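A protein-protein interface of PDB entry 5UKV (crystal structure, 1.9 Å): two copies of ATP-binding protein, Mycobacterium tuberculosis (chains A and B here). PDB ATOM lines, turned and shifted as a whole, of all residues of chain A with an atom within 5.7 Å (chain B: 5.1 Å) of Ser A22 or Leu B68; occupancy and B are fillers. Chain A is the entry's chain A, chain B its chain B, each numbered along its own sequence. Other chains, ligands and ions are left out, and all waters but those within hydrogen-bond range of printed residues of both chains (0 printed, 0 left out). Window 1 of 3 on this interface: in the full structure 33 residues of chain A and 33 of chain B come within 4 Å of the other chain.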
ATOM      1  N   PHE A  17     -21.642 -16.886  -2.160  1.00  0.00           N
ATOM      2  CA  PHE A  17     -20.875 -17.780  -1.267  1.00  0.00           C
ATOM      3  C   PHE A  17     -19.365 -17.640  -1.626  1.00  0.00           C
ATOM      4  O   PHE A  17     -18.487 -17.444  -0.752  1.00  0.00           O
ATOM      5  CB  PHE A  17     -21.349 -19.196  -1.404  1.00  0.00           C
ATOM      6  CG  PHE A  17     -20.510 -20.159  -0.713  1.00  0.00           C
ATOM      7  CD1 PHE A  17     -20.573 -20.280   0.695  1.00  0.00           C
ATOM      8  CD2 PHE A  17     -19.598 -20.918  -1.404  1.00  0.00           C
ATOM      9  CE1 PHE A  17     -19.733 -21.171   1.351  1.00  0.00           C
ATOM     10  CE2 PHE A  17     -18.757 -21.832  -0.733  1.00  0.00           C
ATOM     11  CZ  PHE A  17     -18.819 -21.929   0.651  1.00  0.00           C
ATOM     12  N   ILE A  18     -19.060 -17.770  -2.910  1.00  0.00           N
ATOM     13  CA  ILE A  18     -17.711 -17.625  -3.388  1.00  0.00           C
ATOM     14  C   ILE A  18     -17.094 -16.226  -3.033  1.00  0.00           C
ATOM     15  O   ILE A  18     -15.928 -16.169  -2.523  1.00  0.00           O
ATOM     16  CB  ILE A  18     -17.589 -18.014  -4.850  1.00  0.00           C
ATOM     17  CG1 ILE A  18     -17.665 -19.465  -4.968  1.00  0.00           C
ATOM     18  CG2 ILE A  18     -16.250 -17.531  -5.390  1.00  0.00           C
ATOM     19  CD1 ILE A  18     -17.939 -20.006  -6.319  1.00  0.00           C
ATOM     20  N   THR A  19     -17.840 -15.134  -3.176  1.00  0.00           N
ATOM     21  CA  THR A  19     -17.353 -13.873  -2.728  1.00  0.00           C
ATOM     22  C   THR A  19     -17.045 -13.808  -1.204  1.00  0.00           C
ATOM     23  O   THR A  19     -16.003 -13.346  -0.817  1.00  0.00           O
ATOM     24  CB  THR A  19     -18.357 -12.814  -3.193  1.00  0.00           C
ATOM     25  OG1 THR A  19     -18.515 -12.964  -4.636  1.00  0.00           O
ATOM     26  CG2 THR A  19     -17.965 -11.473  -2.804  1.00  0.00           C
ATOM     27  N   ASP A  20     -17.995 -14.259  -0.377  1.00  0.00           N
ATOM     28  CA  ASP A  20     -17.770 -14.306   1.077  1.00  0.00           C
ATOM     29  C   ASP A  20     -16.638 -15.128   1.458  1.00  0.00           C
ATOM     30  O   ASP A  20     -15.734 -14.706   2.170  1.00  0.00           O
ATOM     31  CB  ASP A  20     -18.998 -14.690   1.902  1.00  0.00           C
ATOM     32  CG  ASP A  20     -20.159 -13.690   1.716  1.00  0.00           C
ATOM     33  OD1 ASP A  20     -19.942 -12.514   1.253  1.00  0.00           O
ATOM     34  OD2 ASP A  20     -21.364 -14.068   1.968  1.00  0.00           O
ATOM     35  N   ALA A  21     -16.589 -16.312   0.957  1.00  0.00           N
ATOM     36  CA  ALA A  21     -15.482 -17.195   1.297  1.00  0.00           C
ATOM     37  C   ALA A  21     -14.112 -16.682   0.897  1.00  0.00           C
ATOM     38  O   ALA A  21     -13.162 -16.803   1.717  1.00  0.00           O
ATOM     39  CB  ALA A  21     -15.770 -18.517   0.732  1.00  0.00           C
ATOM     40  N   SER A  22     -14.010 -16.029  -0.251  1.00  0.00           N
ATOM     41  CA  SER A  22     -12.813 -15.500  -0.667  1.00  0.00           C
ATOM     42  C   SER A  22     -12.292 -14.289   0.065  1.00  0.00           C
ATOM     43  O   SER A  22     -11.094 -14.262   0.346  1.00  0.00           O
ATOM     44  CB  SER A  22     -12.862 -15.172  -2.118  1.00  0.00           C
ATOM     45  OG  SER A  22     -13.289 -16.327  -2.838  1.00  0.00           O
ATOM     46  N   HIS A  23     -13.194 -13.403   0.467  1.00  0.00           N
ATOM     47  CA  HIS A  23     -12.873 -12.321   1.373  1.00  0.00           C
ATOM     48  C   HIS A  23     -12.442 -12.803   2.722  1.00  0.00           C
ATOM     49  O   HIS A  23     -11.502 -12.238   3.284  1.00  0.00           O
ATOM     50  CB  HIS A  23     -14.047 -11.324   1.499  1.00  0.00           C
ATOM     51  CG  HIS A  23     -14.188 -10.393   0.317  1.00  0.00           C
ATOM     52  ND1 HIS A  23     -13.212  -9.515  -0.066  1.00  0.00           N
ATOM     53  CD2 HIS A  23     -15.246 -10.146  -0.491  1.00  0.00           C
ATOM     54  CE1 HIS A  23     -13.654  -8.789  -1.075  1.00  0.00           C
ATOM     55  NE2 HIS A  23     -14.885  -9.154  -1.352  1.00  0.00           N
ATOM     56  N   GLU A  24     -13.001 -13.907   3.205  1.00  0.00           N
ATOM     57  CA  GLU A  24     -12.565 -14.440   4.469  1.00  0.00           C
ATOM     58  C   GLU A  24     -11.130 -14.997   4.443  1.00  0.00           C
ATOM     59  O   GLU A  24     -10.348 -14.876   5.420  1.00  0.00           O
ATOM     60  CB  GLU A  24     -13.536 -15.592   4.884  1.00  0.00           C
ATOM     61  CG  GLU A  24     -14.909 -15.156   5.480  1.00  0.00           C
ATOM     62  CD  GLU A  24     -15.903 -16.299   5.595  1.00  0.00           C
ATOM     63  OE1 GLU A  24     -15.522 -17.493   5.333  1.00  0.00           O
ATOM     64  OE2 GLU A  24     -17.125 -15.994   5.791  1.00  0.00           O
ATOM     65  N   LEU A  25     -10.748 -15.548   3.295  1.00  0.00           N
ATOM     66  CA  LEU A  25      -9.351 -15.972   3.076  1.00  0.00           C
ATOM     67  C   LEU A  25      -8.420 -14.831   2.930  1.00  0.00           C
ATOM     68  O   LEU A  25      -7.276 -14.895   3.328  1.00  0.00           O
ATOM     69  CB  LEU A  25      -9.256 -16.888   1.814  1.00  0.00           C
ATOM     70  CG  LEU A  25      -9.969 -18.208   1.904  1.00  0.00           C
ATOM     71  CD1 LEU A  25     -10.079 -18.803   0.495  1.00  0.00           C
ATOM     72  CD2 LEU A  25      -9.186 -19.092   2.921  1.00  0.00           C
ATOM     73  N   ARG A  26      -8.894 -13.777   2.326  1.00  0.00           N
ATOM     74  CA  ARG A  26      -8.080 -12.640   2.072  1.00  0.00           C
ATOM     75  C   ARG A  26      -7.517 -11.964   3.282  1.00  0.00           C
ATOM     76  O   ARG A  26      -6.444 -11.483   3.245  1.00  0.00           O
ATOM     77  CB  ARG A  26      -8.854 -11.628   1.283  1.00  0.00           C
ATOM     78  CG  ARG A  26      -8.041 -11.143   0.150  1.00  0.00           C
ATOM     79  CD  ARG A  26      -8.435  -9.757  -0.211  1.00  0.00           C
ATOM     80  NE  ARG A  26      -8.986  -9.707  -1.527  1.00  0.00           N
ATOM     81  CZ  ARG A  26      -9.089  -8.569  -2.187  1.00  0.00           C
ATOM     82  NH1 ARG A  26      -9.608  -8.524  -3.402  1.00  0.00           N
ATOM     83  NH2 ARG A  26      -8.683  -7.459  -1.607  1.00  0.00           N
ATOM     84  N   THR A  27      -8.286 -11.919   4.341  1.00  0.00           N
ATOM     85  CA  THR A  27      -7.874 -11.268   5.505  1.00  0.00           C
ATOM     86  C   THR A  27      -6.642 -11.905   6.187  1.00  0.00           C
ATOM     87  O   THR A  27      -5.668 -11.238   6.348  1.00  0.00           O
ATOM     88  CB  THR A  27      -9.057 -11.158   6.447  1.00  0.00           C
ATOM     89  OG1 THR A  27     -10.139 -10.541   5.732  1.00  0.00           O
ATOM     90  CG2 THR A  27      -8.701 -10.396   7.681  1.00  0.00           C
ATOM     91  N   PHE B  17     -14.324 -24.811  -9.604  1.00  0.00           N
ATOM     92  CA  PHE B  17     -13.273 -23.806  -9.323  1.00  0.00           C
ATOM     93  C   PHE B  17     -12.950 -23.674  -7.903  1.00  0.00           C
ATOM     94  O   PHE B  17     -11.801 -23.585  -7.525  1.00  0.00           O
ATOM     95  CB  PHE B  17     -13.579 -22.425  -9.926  1.00  0.00           C
ATOM     96  CG  PHE B  17     -13.046 -22.300 -11.338  1.00  0.00           C
ATOM     97  CD1 PHE B  17     -11.707 -22.064 -11.572  1.00  0.00           C
ATOM     98  CD2 PHE B  17     -13.920 -22.432 -12.476  1.00  0.00           C
ATOM     99  CE1 PHE B  17     -11.232 -21.987 -12.916  1.00  0.00           C
ATOM    100  CE2 PHE B  17     -13.433 -22.343 -13.801  1.00  0.00           C
ATOM    101  CZ  PHE B  17     -12.095 -22.121 -14.001  1.00  0.00           C
ATOM    102  N   ILE B  18     -13.955 -23.596  -7.082  1.00  0.00           N
ATOM    103  CA  ILE B  18     -13.692 -23.473  -5.690  1.00  0.00           C
ATOM    104  C   ILE B  18     -13.001 -24.735  -5.160  1.00  0.00           C
ATOM    105  O   ILE B  18     -12.102 -24.629  -4.399  1.00  0.00           O
ATOM    106  CB  ILE B  18     -14.861 -22.914  -4.899  1.00  0.00           C
ATOM    107  CG1 ILE B  18     -14.355 -22.486  -3.540  1.00  0.00           C
ATOM    108  CG2 ILE B  18     -15.927 -23.916  -4.767  1.00  0.00           C
ATOM    109  CD1 ILE B  18     -14.975 -21.230  -3.002  1.00  0.00           C
ATOM    110  N   ALA B  21      -9.274 -24.496  -6.600  1.00  0.00           N
ATOM    111  CA  ALA B  21      -8.616 -23.440  -5.816  1.00  0.00           C
ATOM    112  C   ALA B  21      -8.291 -23.834  -4.417  1.00  0.00           C
ATOM    113  O   ALA B  21      -7.181 -23.589  -3.944  1.00  0.00           O
ATOM    114  CB  ALA B  21      -9.426 -22.137  -5.914  1.00  0.00           C
ATOM    115  N   LEU B  64      -4.756 -16.613  -6.509  1.00  0.00           N
ATOM    116  CA  LEU B  64      -5.854 -17.603  -6.458  1.00  0.00           C
ATOM    117  C   LEU B  64      -7.141 -17.071  -5.826  1.00  0.00           C
ATOM    118  O   LEU B  64      -8.265 -17.289  -6.350  1.00  0.00           O
ATOM    119  CB  LEU B  64      -5.386 -18.856  -5.660  1.00  0.00           C
ATOM    120  CG  LEU B  64      -4.401 -19.772  -6.459  1.00  0.00           C
ATOM    121  CD1 LEU B  64      -3.822 -20.814  -5.481  1.00  0.00           C
ATOM    122  CD2 LEU B  64      -5.211 -20.443  -7.546  1.00  0.00           C
ATOM    123  N   VAL B  65      -7.004 -16.409  -4.690  1.00  0.00           N
ATOM    124  CA  VAL B  65      -8.119 -15.787  -4.047  1.00  0.00           C
ATOM    125  C   VAL B  65      -8.784 -14.713  -4.962  1.00  0.00           C
ATOM    126  O   VAL B  65      -9.999 -14.665  -5.119  1.00  0.00           O
ATOM    127  CB  VAL B  65      -7.737 -15.282  -2.650  1.00  0.00           C
ATOM    128  CG1 VAL B  65      -8.870 -14.489  -2.058  1.00  0.00           C
ATOM    129  CG2 VAL B  65      -7.331 -16.521  -1.717  1.00  0.00           C
ATOM    130  N   ASP B  66      -7.995 -13.846  -5.546  1.00  0.00           N
ATOM    131  CA  ASP B  66      -8.542 -12.845  -6.443  1.00  0.00           C
ATOM    132  C   ASP B  66      -9.185 -13.482  -7.662  1.00  0.00           C
ATOM    133  O   ASP B  66     -10.143 -12.945  -8.223  1.00  0.00           O
ATOM    134  CB  ASP B  66      -7.510 -11.848  -6.851  1.00  0.00           C
ATOM    135  CG  ASP B  66      -7.268 -10.811  -5.776  1.00  0.00           C
ATOM    136  OD1 ASP B  66      -7.949 -10.842  -4.715  1.00  0.00           O
ATOM    137  OD2 ASP B  66      -6.373  -9.969  -5.967  1.00  0.00           O
ATOM    138  N   ASP B  67      -8.671 -14.591  -8.133  1.00  0.00           N
ATOM    139  CA  ASP B  67      -9.295 -15.226  -9.272  1.00  0.00           C
ATOM    140  C   ASP B  67     -10.746 -15.644  -8.921  1.00  0.00           C
ATOM    141  O   ASP B  67     -11.604 -15.569  -9.728  1.00  0.00           O
ATOM    142  CB  ASP B  67      -8.535 -16.467  -9.693  1.00  0.00           C
ATOM    143  CG  ASP B  67      -7.285 -16.178 -10.535  1.00  0.00           C
ATOM    144  OD1 ASP B  67      -7.004 -15.063 -10.921  1.00  0.00           O
ATOM    145  OD2 ASP B  67      -6.543 -17.111 -10.796  1.00  0.00           O
ATOM    146  N   LEU B  68     -10.951 -16.152  -7.713  1.00  0.00           N
ATOM    147  CA  LEU B  68     -12.244 -16.568  -7.252  1.00  0.00           C
ATOM    148  C   LEU B  68     -13.175 -15.377  -7.171  1.00  0.00           C
ATOM    149  O   LEU B  68     -14.355 -15.438  -7.638  1.00  0.00           O
ATOM    150  CB  LEU B  68     -12.183 -17.201  -5.851  1.00  0.00           C
ATOM    151  CG  LEU B  68     -11.628 -18.601  -5.683  1.00  0.00           C
ATOM    152  CD1 LEU B  68     -11.368 -19.093  -4.245  1.00  0.00           C
ATOM    153  CD2 LEU B  68     -12.579 -19.564  -6.342  1.00  0.00           C
ATOM    154  N   LEU B  69     -12.693 -14.329  -6.526  1.00  0.00           N
ATOM    155  CA  LEU B  69     -13.506 -13.135  -6.408  1.00  0.00           C
ATOM    156  C   LEU B  69     -13.928 -12.642  -7.825  1.00  0.00           C
ATOM    157  O   LEU B  69     -15.012 -12.145  -8.001  1.00  0.00           O
ATOM    158  CB  LEU B  69     -12.778 -12.012  -5.622  1.00  0.00           C
ATOM    159  CG  LEU B  69     -12.566 -12.193  -4.078  1.00  0.00           C
ATOM    160  CD1 LEU B  69     -11.547 -11.252  -3.429  1.00  0.00           C
ATOM    161  CD2 LEU B  69     -13.880 -11.903  -3.324  1.00  0.00           C
ATOM    162  N   LEU B  70     -13.034 -12.684  -8.777  1.00  0.00           N
ATOM    163  CA  LEU B  70     -13.374 -12.150 -10.085  1.00  0.00           C
ATOM    164  C   LEU B  70     -14.347 -13.083 -10.831  1.00  0.00           C
ATOM    165  O   LEU B  70     -15.273 -12.672 -11.556  1.00  0.00           O
ATOM    166  CB  LEU B  70     -12.076 -12.056 -10.914  1.00  0.00           C
ATOM    167  CG  LEU B  70     -12.284 -11.574 -12.374  1.00  0.00           C
ATOM    168  CD1 LEU B  70     -12.899 -10.183 -12.380  1.00  0.00           C
ATOM    169  CD2 LEU B  70     -11.002 -11.674 -13.063  1.00  0.00           C
ATOM    170  N   LEU B  71     -14.109 -14.375 -10.671  1.00  0.00           N
ATOM    171  CA  LEU B  71     -15.046 -15.345 -11.223  1.00  0.00           C
ATOM    172  C   LEU B  71     -16.446 -15.141 -10.782  1.00  0.00           C
ATOM    173  O   LEU B  71     -17.354 -15.155 -11.615  1.00  0.00           O
ATOM    174  CB  LEU B  71     -14.641 -16.758 -10.824  1.00  0.00           C
ATOM    175  CG  LEU B  71     -15.534 -17.922 -11.194  1.00  0.00           C
ATOM    176  CD1 LEU B  71     -15.229 -18.174 -12.630  1.00  0.00           C
ATOM    177  CD2 LEU B  71     -15.317 -19.138 -10.302  1.00  0.00           C
ATOM    178  N   ALA B  72     -16.620 -14.879  -9.517  1.00  0.00           N
ATOM    179  CA  ALA B  72     -17.903 -14.554  -8.935  1.00  0.00           C
ATOM    180  C   ALA B  72     -18.556 -13.342  -9.588  1.00  0.00           C
ATOM    181  O   ALA B  72     -19.772 -13.280  -9.631  1.00  0.00           O
ATOM    182  CB  ALA B  72     -17.818 -14.346  -7.424  1.00  0.00           C
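Ile A18 touches Ile B18 (CG1 to CD1, 3.8 Å).
Ile A18 touches Leu B68 (CG2 to O, 3.6 Å).
CD2 of Leu B69 touches O of Thr A19, 3.6 Å away.
Thr A19 touches Ala B72 (OG1 to CB, 3.2 Å).
CG1 of Val B65 touches O of Ser A22, at 3.3 Å.
CB of Leu B68 touches OG of Ser A22, at 3.3 Å.
CB of Ser A22 touches CG of Leu B69 (3.6 Å).
NE2 of His A23 touches CD2 of Leu B69 (3.5 Å).
Arg A26 touches Leu B69 (NH1 to CD1, 3.3 Å).
O of Ile A18 sits at hydrogen-bond distance from OG of Ser A22 (2.7 Å).
O of His A23 sits at hydrogen-bond distance from OG1 of Thr A27 (3.3 Å).
Of the printed residues of chain B, Arg A26 touches Asp B66 and Leu B69.
Of chain A, only Ile A18 (3.6 Å) and Ser A22 (3.3 Å) come within 4 Å of Leu B68.
Printed residues of chain A within 4 Å of Ala B72: Thr A19.
The nearest printed residue of chain B that does not touch Ser A22 is Ile B18 (5.2 Å).
The nearest residue of chain A that does not touch Leu B68 is Leu A25 (4.9 Å).
The guanidinium group (NH1) of Arg A26 lies within salt-bridge range of the side-chain carboxylate (OD1) of Asp B66 (3.1 Å).
Ile A18 touches its own counterpart, Ile B18.
Of the 11 printed residues of chain A, 5 touch a printed residue of chain B.
Hydrophobic or aromatic side chains of chain A within 4 Å of the printed part of chain B: Ile A18 and His A23.
Of the 12 printed residues of chain B, 6 touch a printed residue of chain A.
Hydrophobic or aromatic side chains of chain B within 4 Å of the printed part of chain A: Ile B18, Val B65, Leu B68, Leu B69 and Ala B72.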
